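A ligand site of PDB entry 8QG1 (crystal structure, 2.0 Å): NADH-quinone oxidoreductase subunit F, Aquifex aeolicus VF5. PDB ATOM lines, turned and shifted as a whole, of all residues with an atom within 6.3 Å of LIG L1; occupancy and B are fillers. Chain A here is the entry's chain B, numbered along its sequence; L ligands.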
ATOM      1  N   ILE A 181      29.212  11.741 -32.606  1.00  0.00           N
ATOM      2  CA  ILE A 181      29.324  11.661 -31.155  1.00  0.00           C
ATOM      3  C   ILE A 181      30.247  12.768 -30.624  1.00  0.00           C
ATOM      4  O   ILE A 181      30.198  13.072 -29.440  1.00  0.00           O
ATOM      5  CB  ILE A 181      29.797  10.271 -30.670  1.00  0.00           C
ATOM      6  CG1 ILE A 181      29.579  10.090 -29.170  1.00  0.00           C
ATOM      7  CG2 ILE A 181      31.254  10.008 -31.042  1.00  0.00           C
ATOM      8  CD1 ILE A 181      28.159  10.307 -28.725  1.00  0.00           C
ATOM      9  N   GLY A 197      36.692  10.040 -30.043  1.00  0.00           N
ATOM     10  CA  GLY A 197      35.550  10.707 -29.432  1.00  0.00           C
ATOM     11  C   GLY A 197      34.716   9.762 -28.575  1.00  0.00           C
ATOM     12  O   GLY A 197      33.652   9.314 -28.987  1.00  0.00           O
ATOM     13  N   HIS A 198      35.224   9.449 -27.379  1.00  0.00           N
ATOM     14  CA  HIS A 198      34.540   8.577 -26.441  1.00  0.00           C
ATOM     15  C   HIS A 198      34.005   9.433 -25.296  1.00  0.00           C
ATOM     16  O   HIS A 198      34.790   9.974 -24.513  1.00  0.00           O
ATOM     17  CB  HIS A 198      35.477   7.488 -25.914  1.00  0.00           C
ATOM     18  CG  HIS A 198      35.810   6.429 -26.908  1.00  0.00           C
ATOM     19  ND1 HIS A 198      36.838   5.535 -26.688  1.00  0.00           N
ATOM     20  CD2 HIS A 198      35.285   6.109 -28.097  1.00  0.00           C
ATOM     21  CE1 HIS A 198      36.916   4.711 -27.725  1.00  0.00           C
ATOM     22  NE2 HIS A 198      35.990   5.037 -28.591  1.00  0.00           N
ATOM     23  N   PRO A 199      32.675   9.581 -25.153  1.00  0.00           N
ATOM     24  CA  PRO A 199      32.093  10.302 -24.020  1.00  0.00           C
ATOM     25  C   PRO A 199      32.619   9.804 -22.683  1.00  0.00           C
ATOM     26  O   PRO A 199      32.965   8.627 -22.544  1.00  0.00           O
ATOM     27  CB  PRO A 199      30.590  10.043 -24.138  1.00  0.00           C
ATOM     28  CG  PRO A 199      30.397   9.825 -25.636  1.00  0.00           C
ATOM     29  CD  PRO A 199      31.647   9.103 -26.093  1.00  0.00           C
ATOM     30  N   ARG A 200      32.686  10.716 -21.711  1.00  0.00           N
ATOM     31  CA  ARG A 200      33.086  10.416 -20.344  1.00  0.00           C
ATOM     32  C   ARG A 200      31.828  10.295 -19.490  1.00  0.00           C
ATOM     33  O   ARG A 200      30.828  10.955 -19.755  1.00  0.00           O
ATOM     34  CB  ARG A 200      33.947  11.543 -19.764  1.00  0.00           C
ATOM     35  CG  ARG A 200      35.210  11.871 -20.537  1.00  0.00           C
ATOM     36  CD  ARG A 200      35.840  13.139 -19.970  1.00  0.00           C
ATOM     37  NE  ARG A 200      37.077  13.533 -20.629  1.00  0.00           N
ATOM     38  CZ  ARG A 200      37.755  14.638 -20.354  1.00  0.00           C
ATOM     39  NH1 ARG A 200      38.926  14.860 -20.938  1.00  0.00           N
ATOM     40  NH2 ARG A 200      37.276  15.514 -19.493  1.00  0.00           N
ATOM     41  N   GLU A 345      26.547   5.936 -35.780  1.00  0.00           N
ATOM     42  CA  GLU A 345      27.162   6.935 -34.901  1.00  0.00           C
ATOM     43  C   GLU A 345      27.451   6.465 -33.472  1.00  0.00           C
ATOM     44  O   GLU A 345      28.139   7.187 -32.751  1.00  0.00           O
ATOM     45  CB  GLU A 345      26.310   8.208 -34.852  1.00  0.00           C
ATOM     46  CG  GLU A 345      26.177   8.879 -36.198  1.00  0.00           C
ATOM     47  CD  GLU A 345      27.489   9.180 -36.904  1.00  0.00           C
ATOM     48  OE1 GLU A 345      28.531   9.324 -36.220  1.00  0.00           O
ATOM     49  OE2 GLU A 345      27.479   9.242 -38.146  1.00  0.00           O
ATOM     50  N   THR A 346      26.936   5.311 -33.031  1.00  0.00           N
ATOM     51  CA  THR A 346      27.290   4.816 -31.701  1.00  0.00           C
ATOM     52  C   THR A 346      28.814   4.677 -31.611  1.00  0.00           C
ATOM     53  O   THR A 346      29.438   4.176 -32.534  1.00  0.00           O
ATOM     54  CB  THR A 346      26.559   3.514 -31.358  1.00  0.00           C
ATOM     55  OG1 THR A 346      27.049   3.040 -30.101  1.00  0.00           O
ATOM     56  CG2 THR A 346      26.740   2.434 -32.405  1.00  0.00           C
ATOM     57  N   CYS A 347      29.403   5.129 -30.491  1.00  0.00           N
ATOM     58  CA  CYS A 347      30.843   5.048 -30.326  1.00  0.00           C
ATOM     59  C   CYS A 347      31.266   3.652 -29.844  1.00  0.00           C
ATOM     60  O   CYS A 347      32.434   3.286 -29.990  1.00  0.00           O
ATOM     61  CB  CYS A 347      31.370   6.139 -29.398  1.00  0.00           C
ATOM     62  SG  CYS A 347      31.191   5.782 -27.641  1.00  0.00           S
ATOM     63  N   GLY A 348      30.327   2.892 -29.266  1.00  0.00           N
ATOM     64  CA  GLY A 348      30.507   1.466 -29.030  1.00  0.00           C
ATOM     65  C   GLY A 348      31.019   1.114 -27.629  1.00  0.00           C
ATOM     66  O   GLY A 348      31.179  -0.058 -27.319  1.00  0.00           O
ATOM     67  N   GLN A 349      31.269   2.132 -26.775  1.00  0.00           N
ATOM     68  CA  GLN A 349      31.796   1.911 -25.432  1.00  0.00           C
ATOM     69  C   GLN A 349      30.823   1.094 -24.595  1.00  0.00           C
ATOM     70  O   GLN A 349      31.256   0.298 -23.759  1.00  0.00           O
ATOM     71  CB  GLN A 349      31.988   3.230 -24.675  1.00  0.00           C
ATOM     72  CG  GLN A 349      33.320   3.917 -24.913  1.00  0.00           C
ATOM     73  CD  GLN A 349      33.400   5.139 -24.029  1.00  0.00           C
ATOM     74  OE1 GLN A 349      34.087   5.137 -23.004  1.00  0.00           O
ATOM     75  NE2 GLN A 349      32.637   6.165 -24.380  1.00  0.00           N
ATOM     76  N   CYS A 350      29.519   1.356 -24.760  1.00  0.00           N
ATOM     77  CA  CYS A 350      28.495   0.714 -23.955  1.00  0.00           C
ATOM     78  C   CYS A 350      27.842  -0.396 -24.774  1.00  0.00           C
ATOM     79  O   CYS A 350      27.500  -0.194 -25.941  1.00  0.00           O
ATOM     80  CB  CYS A 350      27.445   1.722 -23.490  1.00  0.00           C
ATOM     81  SG  CYS A 350      28.127   3.319 -22.937  1.00  0.00           S
ATOM     82  N   THR A 351      27.655  -1.564 -24.150  1.00  0.00           N
ATOM     83  CA  THR A 351      27.245  -2.772 -24.859  1.00  0.00           C
ATOM     84  C   THR A 351      25.810  -2.627 -25.380  1.00  0.00           C
ATOM     85  O   THR A 351      25.577  -2.850 -26.555  1.00  0.00           O
ATOM     86  CB  THR A 351      27.486  -4.022 -23.999  1.00  0.00           C
ATOM     87  OG1 THR A 351      28.912  -4.227 -23.956  1.00  0.00           O
ATOM     88  CG2 THR A 351      26.808  -5.269 -24.518  1.00  0.00           C
ATOM     89  N   CYS A 353      24.093   0.003 -26.063  1.00  0.00           N
ATOM     90  CA  CYS A 353      24.112   0.989 -27.132  1.00  0.00           C
ATOM     91  C   CYS A 353      24.802   0.421 -28.380  1.00  0.00           C
ATOM     92  O   CYS A 353      24.291   0.573 -29.485  1.00  0.00           O
ATOM     93  CB  CYS A 353      24.798   2.262 -26.667  1.00  0.00           C
ATOM     94  SG  CYS A 353      24.821   3.594 -27.909  1.00  0.00           S
ATOM     95  N   ARG A 354      25.934  -0.273 -28.192  1.00  0.00           N
ATOM     96  CA  ARG A 354      26.714  -0.782 -29.315  1.00  0.00           C
ATOM     97  C   ARG A 354      25.875  -1.761 -30.130  1.00  0.00           C
ATOM     98  O   ARG A 354      25.747  -1.618 -31.348  1.00  0.00           O
ATOM     99  CB  ARG A 354      28.014  -1.436 -28.829  1.00  0.00           C
ATOM    100  CG  ARG A 354      28.837  -2.098 -29.918  1.00  0.00           C
ATOM    101  CD  ARG A 354      30.128  -2.719 -29.420  1.00  0.00           C
ATOM    102  NE  ARG A 354      29.900  -3.877 -28.559  1.00  0.00           N
ATOM    103  CZ  ARG A 354      30.003  -3.862 -27.236  1.00  0.00           C
ATOM    104  NH1 ARG A 354      30.263  -2.725 -26.608  1.00  0.00           N
ATOM    105  NH2 ARG A 354      29.831  -4.974 -26.542  1.00  0.00           N
ATOM    106  N   CYS A 357      21.985  -0.266 -31.154  1.00  0.00           N
ATOM    107  CA  CYS A 357      21.927   0.620 -32.313  1.00  0.00           C
ATOM    108  C   CYS A 357      22.085  -0.191 -33.597  1.00  0.00           C
ATOM    109  O   CYS A 357      21.364   0.046 -34.571  1.00  0.00           O
ATOM    110  CB  CYS A 357      22.943   1.759 -32.230  1.00  0.00           C
ATOM    111  SG  CYS A 357      22.512   3.023 -31.000  1.00  0.00           S
ATOM    112  N   ILE A 387      18.180  -0.061 -25.612  1.00  0.00           N
ATOM    113  CA  ILE A 387      19.424   0.565 -26.042  1.00  0.00           C
ATOM    114  C   ILE A 387      20.018   1.370 -24.875  1.00  0.00           C
ATOM    115  O   ILE A 387      21.240   1.433 -24.724  1.00  0.00           O
ATOM    116  CB  ILE A 387      19.196   1.449 -27.290  1.00  0.00           C
ATOM    117  CG1 ILE A 387      18.610   0.647 -28.451  1.00  0.00           C
ATOM    118  CG2 ILE A 387      20.479   2.176 -27.680  1.00  0.00           C
ATOM    119  CD1 ILE A 387      18.170   1.477 -29.633  1.00  0.00           C
ATOM    120  N   THR A 390      22.685   1.131 -19.078  1.00  0.00           N
ATOM    121  CA  THR A 390      24.107   1.294 -18.807  1.00  0.00           C
ATOM    122  C   THR A 390      24.760   2.396 -19.647  1.00  0.00           C
ATOM    123  O   THR A 390      25.964   2.620 -19.481  1.00  0.00           O
ATOM    124  CB  THR A 390      24.906  -0.024 -18.949  1.00  0.00           C
ATOM    125  OG1 THR A 390      25.200  -0.261 -20.324  1.00  0.00           O
ATOM    126  CG2 THR A 390      24.185  -1.209 -18.347  1.00  0.00           C
ATOM    127  N   SER A 391      24.013   3.101 -20.504  1.00  0.00           N
ATOM    128  CA  SER A 391      24.600   4.099 -21.382  1.00  0.00           C
ATOM    129  C   SER A 391      25.207   5.234 -20.569  1.00  0.00           C
ATOM    130  O   SER A 391      24.645   5.664 -19.558  1.00  0.00           O
ATOM    131  CB  SER A 391      23.586   4.618 -22.375  1.00  0.00           C
ATOM    132  OG  SER A 391      22.413   5.066 -21.712  1.00  0.00           O
ATOM    133  N   ILE A 392      26.367   5.743 -21.009  1.00  0.00           N
ATOM    134  CA  ILE A 392      27.008   6.833 -20.280  1.00  0.00           C
ATOM    135  C   ILE A 392      26.820   8.180 -20.989  1.00  0.00           C
ATOM    136  O   ILE A 392      27.344   9.171 -20.498  1.00  0.00           O
ATOM    137  CB  ILE A 392      28.495   6.538 -19.980  1.00  0.00           C
ATOM    138  CG1 ILE A 392      29.369   6.449 -21.238  1.00  0.00           C
ATOM    139  CG2 ILE A 392      28.607   5.279 -19.141  1.00  0.00           C
ATOM    140  CD1 ILE A 392      30.726   5.836 -20.998  1.00  0.00           C
ATOM    141  N   CYS A 393      26.089   8.222 -22.107  1.00  0.00           N
ATOM    142  CA  CYS A 393      25.777   9.494 -22.747  1.00  0.00           C
ATOM    143  C   CYS A 393      24.397   9.445 -23.394  1.00  0.00           C
ATOM    144  O   CYS A 393      23.766   8.387 -23.471  1.00  0.00           O
ATOM    145  CB  CYS A 393      26.836   9.934 -23.763  1.00  0.00           C
ATOM    146  SG  CYS A 393      26.557   9.415 -25.479  1.00  0.00           S
ATOM    147  N   GLY A 394      23.942  10.614 -23.852  1.00  0.00           N
ATOM    148  CA  GLY A 394      22.573  10.811 -24.297  1.00  0.00           C
ATOM    149  C   GLY A 394      22.229  10.067 -25.579  1.00  0.00           C
ATOM    150  O   GLY A 394      21.051   9.864 -25.850  1.00  0.00           O
ATOM    151  N   LEU A 395      23.246   9.659 -26.366  1.00  0.00           N
ATOM    152  CA  LEU A 395      22.960   8.947 -27.601  1.00  0.00           C
ATOM    153  C   LEU A 395      22.235   7.640 -27.278  1.00  0.00           C
ATOM    154  O   LEU A 395      21.148   7.392 -27.814  1.00  0.00           O
ATOM    155  CB  LEU A 395      24.257   8.713 -28.392  1.00  0.00           C
ATOM    156  CG  LEU A 395      24.064   8.180 -29.817  1.00  0.00           C
ATOM    157  CD1 LEU A 395      25.201   8.642 -30.724  1.00  0.00           C
ATOM    158  CD2 LEU A 395      23.970   6.654 -29.840  1.00  0.00           C
ATOM    159  N   GLY A 396      22.808   6.836 -26.379  1.00  0.00           N
ATOM    160  CA  GLY A 396      22.184   5.581 -25.990  1.00  0.00           C
ATOM    161  C   GLY A 396      20.796   5.812 -25.379  1.00  0.00           C
ATOM    162  O   GLY A 396      19.891   5.000 -25.561  1.00  0.00           O
ATOM    163  N   ALA A 397      20.633   6.954 -24.703  1.00  0.00           N
ATOM    164  CA  ALA A 397      19.391   7.290 -24.038  1.00  0.00           C
ATOM    165  C   ALA A 397      18.271   7.596 -25.037  1.00  0.00           C
ATOM    166  O   ALA A 397      17.102   7.431 -24.673  1.00  0.00           O
ATOM    167  CB  ALA A 397      19.618   8.424 -23.080  1.00  0.00           C
HETATM  168 FE1  LIG L   1      29.077   5.675 -26.907  1.00  0.00          FE
HETATM  169 FE2  LIG L   1      26.417   4.920 -26.999  1.00  0.00          FE
HETATM  170 FE3  LIG L   1      27.145   7.232 -25.685  1.00  0.00          FE
HETATM  171 FE4  LIG L   1      27.816   4.774 -24.643  1.00  0.00          FE
HETATM  172  S1  LIG L   1      25.684   5.649 -24.916  1.00  0.00           S
HETATM  173  S2  LIG L   1      29.171   6.594 -24.777  1.00  0.00           S
HETATM  174  S3  LIG L   1      28.248   3.572 -26.564  1.00  0.00           S
HETATM  175  S4  LIG L   1      27.362   6.746 -27.972  1.00  0.00           S
HETATM  176  N1  LG2 L   2      25.541  20.260 -28.748  1.00  0.00           N
HETATM  177  C1  LG2 L   2      25.938  21.117 -29.742  1.00  0.00           C
HETATM  178  O1  LG2 L   2      26.133  22.336 -29.525  1.00  0.00           O
HETATM  179  N2  LG2 L   2      26.231  20.609 -31.012  1.00  0.00           N
HETATM  180  C2  LG2 L   2      26.196  19.281 -31.387  1.00  0.00           C
HETATM  181  O2  LG2 L   2      26.520  18.963 -32.535  1.00  0.00           O
HETATM  182  C3  LG2 L   2      25.788  18.361 -30.320  1.00  0.00           C
HETATM  183  N3  LG2 L   2      25.765  17.076 -30.568  1.00  0.00           N
HETATM  184  C4  LG2 L   2      25.415  16.216 -29.531  1.00  0.00           C
HETATM  185  C5  LG2 L   2      25.414  14.837 -29.779  1.00  0.00           C
HETATM  186  C6  LG2 L   2      25.063  13.935 -28.773  1.00  0.00           C
HETATM  187  C7  LG2 L   2      25.045  12.451 -29.083  1.00  0.00           C
HETATM  188  C8  LG2 L   2      24.716  14.407 -27.503  1.00  0.00           C
HETATM  189  C9  LG2 L   2      24.239  13.449 -26.436  1.00  0.00           C
HETATM  190  C10 LG2 L   2      24.719  15.766 -27.249  1.00  0.00           C
HETATM  191  C11 LG2 L   2      25.061  16.679 -28.251  1.00  0.00           C
HETATM  192  N4  LG2 L   2      25.101  18.085 -28.028  1.00  0.00           N
HETATM  193  C12 LG2 L   2      25.468  18.960 -29.026  1.00  0.00           C
HETATM  194  C13 LG2 L   2      24.823  18.636 -26.698  1.00  0.00           C
HETATM  195  C14 LG2 L   2      26.133  18.854 -25.962  1.00  0.00           C
HETATM  196  O3  LG2 L   2      26.527  17.649 -25.303  1.00  0.00           O
HETATM  197  C15 LG2 L   2      25.988  19.991 -24.949  1.00  0.00           C
HETATM  198  O4  LG2 L   2      24.784  19.810 -24.198  1.00  0.00           O
HETATM  199  C16 LG2 L   2      25.959  21.389 -25.578  1.00  0.00           C
HETATM  200  O5  LG2 L   2      27.022  21.560 -26.513  1.00  0.00           O
HETATM  201  C17 LG2 L   2      26.027  22.466 -24.519  1.00  0.00           C
HETATM  202  O6  LG2 L   2      25.837  23.776 -25.111  1.00  0.00           O
HETATM  203  P1  LG2 L   2      24.456  24.573 -24.806  1.00  0.00           P
HETATM  204  O7  LG2 L   2      24.772  25.967 -25.294  1.00  0.00           O
HETATM  205  O8  LG2 L   2      23.362  23.885 -25.593  1.00  0.00           O
HETATM  206  O9  LG2 L   2      24.198  24.546 -23.310  1.00  0.00           O
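Residues that only touch LIG L1: Ile 181, Pro 199, Ser 391, Ile 392 and Leu 395. Hydrophobic or aromatic side chains within 4 Å of LIG L1: Ile 181, Pro 199, Ile 392 and Leu 395. The nearest printed residue that does not touch LIG L1 is Arg 354 (4.8 Å).
S4 of LIG L1 lies close to N of Cys 347, at 3.6 Å. SG of Cys 347 binds FE1 of LIG L1 (2.2 Å). The backbone NH (N) of Cys 350 sits close to a sulfur (S3) of LIG L1 (3.1 Å). FE4 of LIG L1 is bound by SG of Cys 350 (2.3 Å). FE2 of LIG L1 is bound by SG of Cys 353 (2.3 Å). The side-chain sulfur (SG) of Cys 393 is bound to an iron atom (FE3) of LIG L1, at 2.3 Å. N of Gln 349 lies close to S3 of LIG L1, at 3.4 Å. The side-chain amide nitrogen (NE2) of Gln 349 lies close to a sulfur (S2) of LIG L1 (3.5 Å). N of Gly 396 lies close to S1 of LIG L1 (3.4 Å). A sulfur (S3) of LIG L1 lies close to the backbone NH (N) of Gly 348 (3.5 Å). A sulfur (S3) of LIG L1 sits close to the side-chain hydroxyl (OG1) of Thr 346 (3.8 Å).
The side-chain sulfur of Cys 347 lies close to the side-chain amide nitrogen of Gln 349, 3.6 Å away. The backbone NH (N) of Ile 392 lies close to the side-chain sulfur (SG) of Cys 350, 3.6 Å away. O of Cys 353 lies close to SG of Cys 357 (3.4 Å). The backbone NH (N) of Cys 353 sits at hydrogen-bond distance from the backbone carbonyl oxygen (O) of Ile 387, 3.5 Å away. SG of Cys 393 lies close to N of Leu 395 (3.4 Å). The side-chain amide nitrogen of Gln 349 is in hydrogen-bond range of the backbone carbonyl oxygen of Pro 199 (3.1 Å). OG1 of Thr 346 lies close to N of Gly 348 (3.4 Å). The backbone carbonyl oxygen (O) of Gly 348 sits at hydrogen-bond distance from the guanidinium group (NH1) of Arg 354 (2.9 Å).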
